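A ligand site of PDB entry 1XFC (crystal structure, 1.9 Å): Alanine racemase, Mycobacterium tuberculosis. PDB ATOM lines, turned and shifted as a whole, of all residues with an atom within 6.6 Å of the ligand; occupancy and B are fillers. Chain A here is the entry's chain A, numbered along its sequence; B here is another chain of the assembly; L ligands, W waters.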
ATOM      1  N   VAL A  40      16.122   0.388  29.598  1.00  0.00           N
ATOM      2  CA  VAL A  40      15.170   0.944  30.578  1.00  0.00           C
ATOM      3  C   VAL A  40      15.510   0.483  31.994  1.00  0.00           C
ATOM      4  O   VAL A  40      15.536  -0.705  32.286  1.00  0.00           O
ATOM      5  CB  VAL A  40      13.724   0.568  30.190  1.00  0.00           C
ATOM      6  CG1 VAL A  40      12.728   1.123  31.201  1.00  0.00           C
ATOM      7  CG2 VAL A  40      13.416   1.090  28.791  1.00  0.00           C
ATOM      8  N   LYS A  42      14.141   2.023  34.902  1.00  0.00           N
ATOM      9  CA  LYS A  42      13.177   2.489  35.903  1.00  0.00           C
ATOM     10  C   LYS A  42      13.028   1.488  37.046  1.00  0.00           C
ATOM     11  O   LYS A  42      13.552   0.371  36.960  1.00  0.00           O
ATOM     12  CB  LYS A  42      11.837   2.757  35.208  1.00  0.00           C
ATOM     13  CG  LYS A  42      11.058   1.506  34.844  1.00  0.00           C
ATOM     14  CD  LYS A  42       9.814   1.869  34.050  1.00  0.00           C
ATOM     15  CE  LYS A  42       9.031   0.676  33.577  1.00  0.00           C
ATOM     16  NZ  LYS A  42       8.471   0.834  32.201  1.00  0.00           N
ATOM     17  N   TYR A  46      14.583  -2.275  37.704  1.00  0.00           N
ATOM     18  CA  TYR A  46      13.719  -3.447  37.872  1.00  0.00           C
ATOM     19  C   TYR A  46      14.179  -4.268  39.077  1.00  0.00           C
ATOM     20  O   TYR A  46      14.157  -5.500  39.005  1.00  0.00           O
ATOM     21  CB  TYR A  46      13.693  -4.372  36.654  1.00  0.00           C
ATOM     22  CG  TYR A  46      12.884  -3.925  35.448  1.00  0.00           C
ATOM     23  CD1 TYR A  46      12.809  -2.571  35.114  1.00  0.00           C
ATOM     24  CD2 TYR A  46      12.218  -4.817  34.621  1.00  0.00           C
ATOM     25  CE1 TYR A  46      12.108  -2.127  34.018  1.00  0.00           C
ATOM     26  CE2 TYR A  46      11.492  -4.389  33.511  1.00  0.00           C
ATOM     27  CZ  TYR A  46      11.441  -3.036  33.225  1.00  0.00           C
ATOM     28  OH  TYR A  46      10.733  -2.582  32.145  1.00  0.00           O
ATOM     29  N   ALA A  68      11.223   6.183  34.215  1.00  0.00           N
ATOM     30  CA  ALA A  68       9.901   6.797  34.289  1.00  0.00           C
ATOM     31  C   ALA A  68       9.997   8.231  34.794  1.00  0.00           C
ATOM     32  O   ALA A  68       9.526   9.183  34.173  1.00  0.00           O
ATOM     33  CB  ALA A  68       8.974   6.007  35.208  1.00  0.00           C
ATOM     34  N   TRP A  88       9.609   9.887  31.328  1.00  0.00           N
ATOM     35  CA  TRP A  88       8.337   9.974  30.630  1.00  0.00           C
ATOM     36  C   TRP A  88       7.086   9.944  31.494  1.00  0.00           C
ATOM     37  O   TRP A  88       5.973   9.966  30.950  1.00  0.00           O
ATOM     38  CB  TRP A  88       8.251   8.799  29.638  1.00  0.00           C
ATOM     39  CG  TRP A  88       8.449   7.425  30.184  1.00  0.00           C
ATOM     40  CD1 TRP A  88       7.670   6.699  31.044  1.00  0.00           C
ATOM     41  CD2 TRP A  88       9.559   6.569  29.872  1.00  0.00           C
ATOM     42  NE1 TRP A  88       8.217   5.463  31.307  1.00  0.00           N
ATOM     43  CE2 TRP A  88       9.381   5.360  30.579  1.00  0.00           C
ATOM     44  CE3 TRP A  88      10.682   6.725  29.065  1.00  0.00           C
ATOM     45  CZ2 TRP A  88      10.304   4.311  30.505  1.00  0.00           C
ATOM     46  CZ3 TRP A  88      11.586   5.674  28.984  1.00  0.00           C
ATOM     47  CH2 TRP A  88      11.393   4.483  29.700  1.00  0.00           C
ATOM     48  N   LYS A 133       5.209  11.724  23.615  1.00  0.00           N
ATOM     49  CA  LYS A 133       4.628  10.403  23.805  1.00  0.00           C
ATOM     50  C   LYS A 133       3.179  10.431  23.322  1.00  0.00           C
ATOM     51  O   LYS A 133       2.356  11.136  23.917  1.00  0.00           O
ATOM     52  CB  LYS A 133       4.730   9.944  25.252  1.00  0.00           C
ATOM     53  CG  LYS A 133       4.325   8.527  25.586  1.00  0.00           C
ATOM     54  CD  LYS A 133       4.747   8.243  27.036  1.00  0.00           C
ATOM     55  CE  LYS A 133       4.737   6.748  27.339  1.00  0.00           C
ATOM     56  NZ  LYS A 133       3.387   6.291  27.764  1.00  0.00           N
ATOM     57  N   MET A 170       7.435   8.910  20.487  1.00  0.00           N
ATOM     58  CA  MET A 170       7.454   7.568  21.072  1.00  0.00           C
ATOM     59  C   MET A 170       6.041   7.138  21.380  1.00  0.00           C
ATOM     60  O   MET A 170       5.112   7.939  21.543  1.00  0.00           O
ATOM     61  CB  MET A 170       8.321   7.525  22.331  1.00  0.00           C
ATOM     62  CG  MET A 170       7.659   8.143  23.549  1.00  0.00           C
ATOM     63  SD  MET A 170       8.664   8.181  25.044  1.00  0.00           S
ATOM     64  CE  MET A 170       8.386   6.513  25.649  1.00  0.00           C
ATOM     65  N   SER A 171       5.843   5.815  21.443  1.00  0.00           N
ATOM     66  CA  SER A 171       4.572   5.288  21.929  1.00  0.00           C
ATOM     67  C   SER A 171       4.894   3.934  22.566  1.00  0.00           C
ATOM     68  O   SER A 171       6.058   3.543  22.469  1.00  0.00           O
ATOM     69  CB  SER A 171       3.483   5.175  20.883  1.00  0.00           C
ATOM     70  OG  SER A 171       2.221   4.970  21.559  1.00  0.00           O
ATOM     71  N   HIS A 172       3.952   3.294  23.222  1.00  0.00           N
ATOM     72  CA  HIS A 172       4.243   2.068  23.970  1.00  0.00           C
ATOM     73  C   HIS A 172       3.190   0.988  23.697  1.00  0.00           C
ATOM     74  O   HIS A 172       1.998   1.276  23.829  1.00  0.00           O
ATOM     75  CB  HIS A 172       4.303   2.383  25.463  1.00  0.00           C
ATOM     76  CG  HIS A 172       4.842   1.322  26.372  1.00  0.00           C
ATOM     77  ND1 HIS A 172       6.030   0.662  26.155  1.00  0.00           N
ATOM     78  CD2 HIS A 172       4.344   0.807  27.518  1.00  0.00           C
ATOM     79  CE1 HIS A 172       6.244  -0.218  27.116  1.00  0.00           C
ATOM     80  NE2 HIS A 172       5.229  -0.151  27.965  1.00  0.00           N
ATOM     81  N   SER A 211       9.174   0.269  20.233  1.00  0.00           N
ATOM     82  CA  SER A 211       9.553  -1.057  20.719  1.00  0.00           C
ATOM     83  C   SER A 211      10.067  -1.234  22.135  1.00  0.00           C
ATOM     84  O   SER A 211      11.116  -0.728  22.524  1.00  0.00           O
ATOM     85  CB  SER A 211      10.669  -1.549  19.749  1.00  0.00           C
ATOM     86  OG  SER A 211      10.127  -1.585  18.417  1.00  0.00           O
ATOM     87  N   ASN A 212       9.307  -2.012  22.899  1.00  0.00           N
ATOM     88  CA  ASN A 212       9.740  -2.576  24.181  1.00  0.00           C
ATOM     89  C   ASN A 212      10.473  -3.893  23.955  1.00  0.00           C
ATOM     90  O   ASN A 212      10.757  -4.270  22.805  1.00  0.00           O
ATOM     91  CB  ASN A 212       8.537  -2.781  25.091  1.00  0.00           C
ATOM     92  CG  ASN A 212       7.464  -3.661  24.475  1.00  0.00           C
ATOM     93  OD1 ASN A 212       7.631  -4.308  23.428  1.00  0.00           O
ATOM     94  ND2 ASN A 212       6.311  -3.680  25.142  1.00  0.00           N
ATOM     95  N   SER A 213      10.816  -4.633  25.003  1.00  0.00           N
ATOM     96  CA  SER A 213      11.591  -5.864  24.845  1.00  0.00           C
ATOM     97  C   SER A 213      10.939  -6.868  23.892  1.00  0.00           C
ATOM     98  O   SER A 213      11.562  -7.404  22.979  1.00  0.00           O
ATOM     99  CB  SER A 213      11.761  -6.566  26.190  1.00  0.00           C
ATOM    100  OG  SER A 213      12.661  -5.836  27.000  1.00  0.00           O
ATOM    101  N   SER A 214       9.658  -7.124  24.133  1.00  0.00           N
ATOM    102  CA  SER A 214       8.879  -8.017  23.320  1.00  0.00           C
ATOM    103  C   SER A 214       8.895  -7.669  21.840  1.00  0.00           C
ATOM    104  O   SER A 214       9.119  -8.491  20.953  1.00  0.00           O
ATOM    105  CB  SER A 214       7.426  -7.975  23.835  1.00  0.00           C
ATOM    106  OG  SER A 214       6.635  -8.832  23.045  1.00  0.00           O
ATOM    107  N   ARG A 228      13.510   0.405  23.237  1.00  0.00           N
ATOM    108  CA  ARG A 228      13.551   0.672  24.675  1.00  0.00           C
ATOM    109  C   ARG A 228      13.274  -0.588  25.479  1.00  0.00           C
ATOM    110  O   ARG A 228      12.180  -0.703  26.041  1.00  0.00           O
ATOM    111  CB  ARG A 228      12.512   1.703  25.103  1.00  0.00           C
ATOM    112  CG  ARG A 228      12.317   2.930  24.248  1.00  0.00           C
ATOM    113  CD  ARG A 228      11.372   3.906  24.968  1.00  0.00           C
ATOM    114  NE  ARG A 228      10.086   3.225  25.216  1.00  0.00           N
ATOM    115  CZ  ARG A 228       9.198   3.169  24.224  1.00  0.00           C
ATOM    116  NH1 ARG A 228       9.501   3.749  23.068  1.00  0.00           N
ATOM    117  NH2 ARG A 228       8.030   2.572  24.377  1.00  0.00           N
ATOM    118  N   PRO A 229      14.183  -1.548  25.508  1.00  0.00           N
ATOM    119  CA  PRO A 229      13.898  -2.808  26.223  1.00  0.00           C
ATOM    120  C   PRO A 229      14.166  -2.638  27.704  1.00  0.00           C
ATOM    121  O   PRO A 229      15.181  -2.015  28.048  1.00  0.00           O
ATOM    122  CB  PRO A 229      14.912  -3.768  25.597  1.00  0.00           C
ATOM    123  CG  PRO A 229      16.081  -2.896  25.227  1.00  0.00           C
ATOM    124  CD  PRO A 229      15.521  -1.547  24.895  1.00  0.00           C
ATOM    125  N   GLY A 230      13.305  -3.172  28.544  1.00  0.00           N
ATOM    126  CA  GLY A 230      13.642  -3.198  29.970  1.00  0.00           C
ATOM    127  C   GLY A 230      13.855  -4.653  30.384  1.00  0.00           C
ATOM    128  O   GLY A 230      14.976  -5.067  30.649  1.00  0.00           O
ATOM    129  N   ILE A 231      12.761  -5.394  30.429  1.00  0.00           N
ATOM    130  CA  ILE A 231      12.712  -6.751  30.969  1.00  0.00           C
ATOM    131  C   ILE A 231      13.796  -7.646  30.374  1.00  0.00           C
ATOM    132  O   ILE A 231      14.450  -8.377  31.121  1.00  0.00           O
ATOM    133  CB  ILE A 231      11.295  -7.327  30.793  1.00  0.00           C
ATOM    134  CG1 ILE A 231      10.968  -8.499  31.734  1.00  0.00           C
ATOM    135  CG2 ILE A 231      11.001  -7.707  29.358  1.00  0.00           C
ATOM    136  CD1 ILE A 231      11.318  -8.231  33.183  1.00  0.00           C
ATOM    137  N   ALA A 232      14.060  -7.627  29.064  1.00  0.00           N
ATOM    138  CA  ALA A 232      15.116  -8.470  28.476  1.00  0.00           C
ATOM    139  C   ALA A 232      16.516  -8.035  28.860  1.00  0.00           C
ATOM    140  O   ALA A 232      17.433  -8.863  28.818  1.00  0.00           O
ATOM    141  CB  ALA A 232      14.983  -8.509  26.954  1.00  0.00           C
ATOM    142  N   TYR A 234      17.403  -7.422  31.869  1.00  0.00           N
ATOM    143  CA  TYR A 234      17.597  -8.259  33.042  1.00  0.00           C
ATOM    144  C   TYR A 234      17.547  -9.736  32.729  1.00  0.00           C
ATOM    145  O   TYR A 234      17.643 -10.553  33.652  1.00  0.00           O
ATOM    146  CB  TYR A 234      16.516  -7.883  34.081  1.00  0.00           C
ATOM    147  CG  TYR A 234      16.528  -6.347  34.124  1.00  0.00           C
ATOM    148  CD1 TYR A 234      17.556  -5.719  34.790  1.00  0.00           C
ATOM    149  CD2 TYR A 234      15.553  -5.613  33.482  1.00  0.00           C
ATOM    150  CE1 TYR A 234      17.636  -4.340  34.853  1.00  0.00           C
ATOM    151  CE2 TYR A 234      15.622  -4.212  33.540  1.00  0.00           C
ATOM    152  CZ  TYR A 234      16.639  -3.603  34.212  1.00  0.00           C
ATOM    153  OH  TYR A 234      16.727  -2.232  34.283  1.00  0.00           O
ATOM    154  N   PRO A 238      10.790 -11.736  27.511  1.00  0.00           N
ATOM    155  CA  PRO A 238       9.709 -10.808  27.131  1.00  0.00           C
ATOM    156  C   PRO A 238       8.502 -11.537  26.555  1.00  0.00           C
ATOM    157  O   PRO A 238       7.405 -11.006  26.455  1.00  0.00           O
ATOM    158  CB  PRO A 238      10.342  -9.920  26.065  1.00  0.00           C
ATOM    159  CG  PRO A 238      11.621 -10.559  25.667  1.00  0.00           C
ATOM    160  CD  PRO A 238      11.974 -11.618  26.667  1.00  0.00           C
ATOM    161  N   TYR A 364       8.269  -9.735  36.243  1.00  0.00           N
ATOM    162  CA  TYR A 364       8.538  -8.331  36.534  1.00  0.00           C
ATOM    163  C   TYR A 364       8.302  -8.059  38.021  1.00  0.00           C
ATOM    164  O   TYR A 364       9.010  -7.341  38.719  1.00  0.00           O
ATOM    165  CB  TYR A 364       7.602  -7.397  35.783  1.00  0.00           C
ATOM    166  CG  TYR A 364       7.599  -7.293  34.285  1.00  0.00           C
ATOM    167  CD1 TYR A 364       7.143  -8.330  33.472  1.00  0.00           C
ATOM    168  CD2 TYR A 364       8.055  -6.136  33.678  1.00  0.00           C
ATOM    169  CE1 TYR A 364       7.150  -8.194  32.083  1.00  0.00           C
ATOM    170  CE2 TYR A 364       8.073  -5.989  32.313  1.00  0.00           C
ATOM    171  CZ  TYR A 364       7.608  -7.025  31.520  1.00  0.00           C
ATOM    172  OH  TYR A 364       7.634  -6.856  30.157  1.00  0.00           O
ATOM    173  N   MET B 319       3.845  -1.702  36.515  1.00  0.00           N
ATOM    174  CA  MET B 319       4.935  -1.681  37.491  1.00  0.00           C
ATOM    175  C   MET B 319       4.963  -0.395  38.309  1.00  0.00           C
ATOM    176  O   MET B 319       5.382  -0.440  39.474  1.00  0.00           O
ATOM    177  CB  MET B 319       6.276  -1.882  36.772  1.00  0.00           C
ATOM    178  CG  MET B 319       7.486  -1.713  37.691  1.00  0.00           C
ATOM    179  SD  MET B 319       9.016  -1.920  36.763  1.00  0.00           S
ATOM    180  CE  MET B 319       9.025  -3.702  36.575  1.00  0.00           C
ATOM    181  N   ASP B 320       4.564   0.732  37.717  1.00  0.00           N
ATOM    182  CA  ASP B 320       4.687   2.019  38.429  1.00  0.00           C
ATOM    183  C   ASP B 320       3.427   2.862  38.302  1.00  0.00           C
ATOM    184  O   ASP B 320       3.466   4.064  38.583  1.00  0.00           O
ATOM    185  CB  ASP B 320       5.895   2.801  37.894  1.00  0.00           C
ATOM    186  CG  ASP B 320       5.735   3.089  36.407  1.00  0.00           C
ATOM    187  OD1 ASP B 320       4.745   2.614  35.806  1.00  0.00           O
ATOM    188  OD2 ASP B 320       6.567   3.794  35.828  1.00  0.00           O
ATOM    189  N   GLN B 321       2.305   2.259  37.925  1.00  0.00           N
ATOM    190  CA  GLN B 321       1.054   3.008  37.818  1.00  0.00           C
ATOM    191  C   GLN B 321      -0.180   2.131  37.696  1.00  0.00           C
ATOM    192  O   GLN B 321      -0.032   0.975  37.286  1.00  0.00           O
ATOM    193  CB  GLN B 321       1.142   3.876  36.553  1.00  0.00           C
ATOM    194  CG  GLN B 321       1.282   3.047  35.278  1.00  0.00           C
ATOM    195  CD  GLN B 321       1.562   3.941  34.069  1.00  0.00           C
ATOM    196  OE1 GLN B 321       2.714   4.148  33.701  1.00  0.00           O
ATOM    197  NE2 GLN B 321       0.497   4.484  33.472  1.00  0.00           N
HETATM  198  N1  LIG L   1       9.009   1.870  27.447  1.00  0.00           N
HETATM  199  C1  LIG L   1       8.235   2.440  28.411  1.00  0.00           C
HETATM  200  C2  LIG L   1       7.523   3.775  28.168  1.00  0.00           C
HETATM  201  C3  LIG L   1       8.084   1.804  29.603  1.00  0.00           C
HETATM  202  O1  LIG L   1       7.308   2.356  30.576  1.00  0.00           O
HETATM  203  C4  LIG L   1       8.704   0.603  29.865  1.00  0.00           C
HETATM  204  C5  LIG L   1       8.492  -0.056  31.241  1.00  0.00           C
HETATM  205  C6  LIG L   1       9.487   0.011  28.881  1.00  0.00           C
HETATM  206  C7  LIG L   1       9.636   0.692  27.687  1.00  0.00           C
HETATM  207  C8  LIG L   1      10.184  -1.323  29.080  1.00  0.00           C
HETATM  208  O2  LIG L   1       9.270  -2.362  28.721  1.00  0.00           O
HETATM  209  P1  LIG L   1       9.629  -3.903  28.805  1.00  0.00           P
HETATM  210  O3  LIG L   1      10.237  -4.056  30.138  1.00  0.00           O
HETATM  211  O4  LIG L   1       8.410  -4.681  28.571  1.00  0.00           O
HETATM  212  O5  LIG L   1      10.673  -4.116  27.744  1.00  0.00           O
HETATM  213  O   HOH W   1       6.581   3.926  33.240  1.00  0.00           O
HETATM  214  O   HOH W   2       8.405  -6.433  26.627  1.00  0.00           O
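Val 40 touches the ligand (CG2 to C7, 3.96 Å). Met 170 touches the ligand. Asn 212 touches the ligand (CB to O5, 3.7 Å). Pro 229 touches the ligand. Hydrophobic or aromatic side chains within 4 Å of the ligand: Val 40, Tyr 46, Trp 88, Met 170, His 172, Ile 231 and Tyr 364. Of the 24 residues printed, 13 come within 4 Å of the ligand. The nearest printed residue that does not touch the ligand is Lys 133 (4.2 Å).
O1 of the ligand sits at hydrogen-bond distance from NE1 of Trp 88, 3.3 Å away. The backbone NH of Ser 213 sits at hydrogen-bond distance from an oxygen (O5) of the ligand (2.8 Å). A nitrogen (N1) of the ligand lies within hydrogen-bond range of a ring nitrogen (ND1) of His 172, 3.5 Å away. The side-chain hydroxyl (OH) of Tyr 364 sits at hydrogen-bond distance from an oxygen (O4) of the ligand (2.8 Å). The guanidinium group (NE) of Arg 228 lies within hydrogen-bond range of a nitrogen (N1) of the ligand. C5 of the ligand is covalently linked to NZ of Lys 42 (1.3 Å). N of Ile 231 sits at hydrogen-bond distance from O3 of the ligand, at 2.9 Å. The side-chain hydroxyl (OH) of Tyr 46 is in hydrogen-bond range of an oxygen (O3) of the ligand (2.5 Å). The side-chain hydroxyl of Ser 213 lies within hydrogen-bond range of an oxygen (O5) of the ligand (2.7 Å). The backbone NH (N) of Gly 230 sits at hydrogen-bond distance from an oxygen (O5) of the ligand, 2.9 Å away.
Water W2 lies within hydrogen-bond range of an oxygen (O4) of the ligand (2.6 Å), the backbone NH (N) of Ser 214 (2.9 Å) and the backbone NH (N) of Ser 213 (3.4 Å). Water W1 lies within hydrogen-bond range of OD2 of Asp 320 of chain B (2.6 Å), NE1 of Trp 88 (3.0 Å) and O1 of the ligand (3.2 Å).
The guanidinium group (NH2) of Arg 228 sits at hydrogen-bond distance from the backbone carbonyl oxygen (O) of Ser 171 (2.9 Å). The backbone NH (N) of Val 40 lies within hydrogen-bond range of the backbone carbonyl oxygen (O) of Pro 229 (3.0 Å). OG of Ser 213 sits at hydrogen-bond distance from N of Ala 232, 3.1 Å away. The guanidinium group (NH2) of Arg 228 sits at hydrogen-bond distance from a ring nitrogen (ND1) of His 172. The backbone carbonyl oxygen (O) of Ser 211 is in hydrogen-bond range of the backbone NH (N) of Arg 228, at 2.7 Å. The side-chain hydroxyl (OG) of Ser 213 sits at hydrogen-bond distance from the backbone NH (N) of Gly 230. N of Trp 88 sits at hydrogen-bond distance from O of Ala 68 (2.9 Å). N of Ile 231 lies close to OG of Ser 213.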
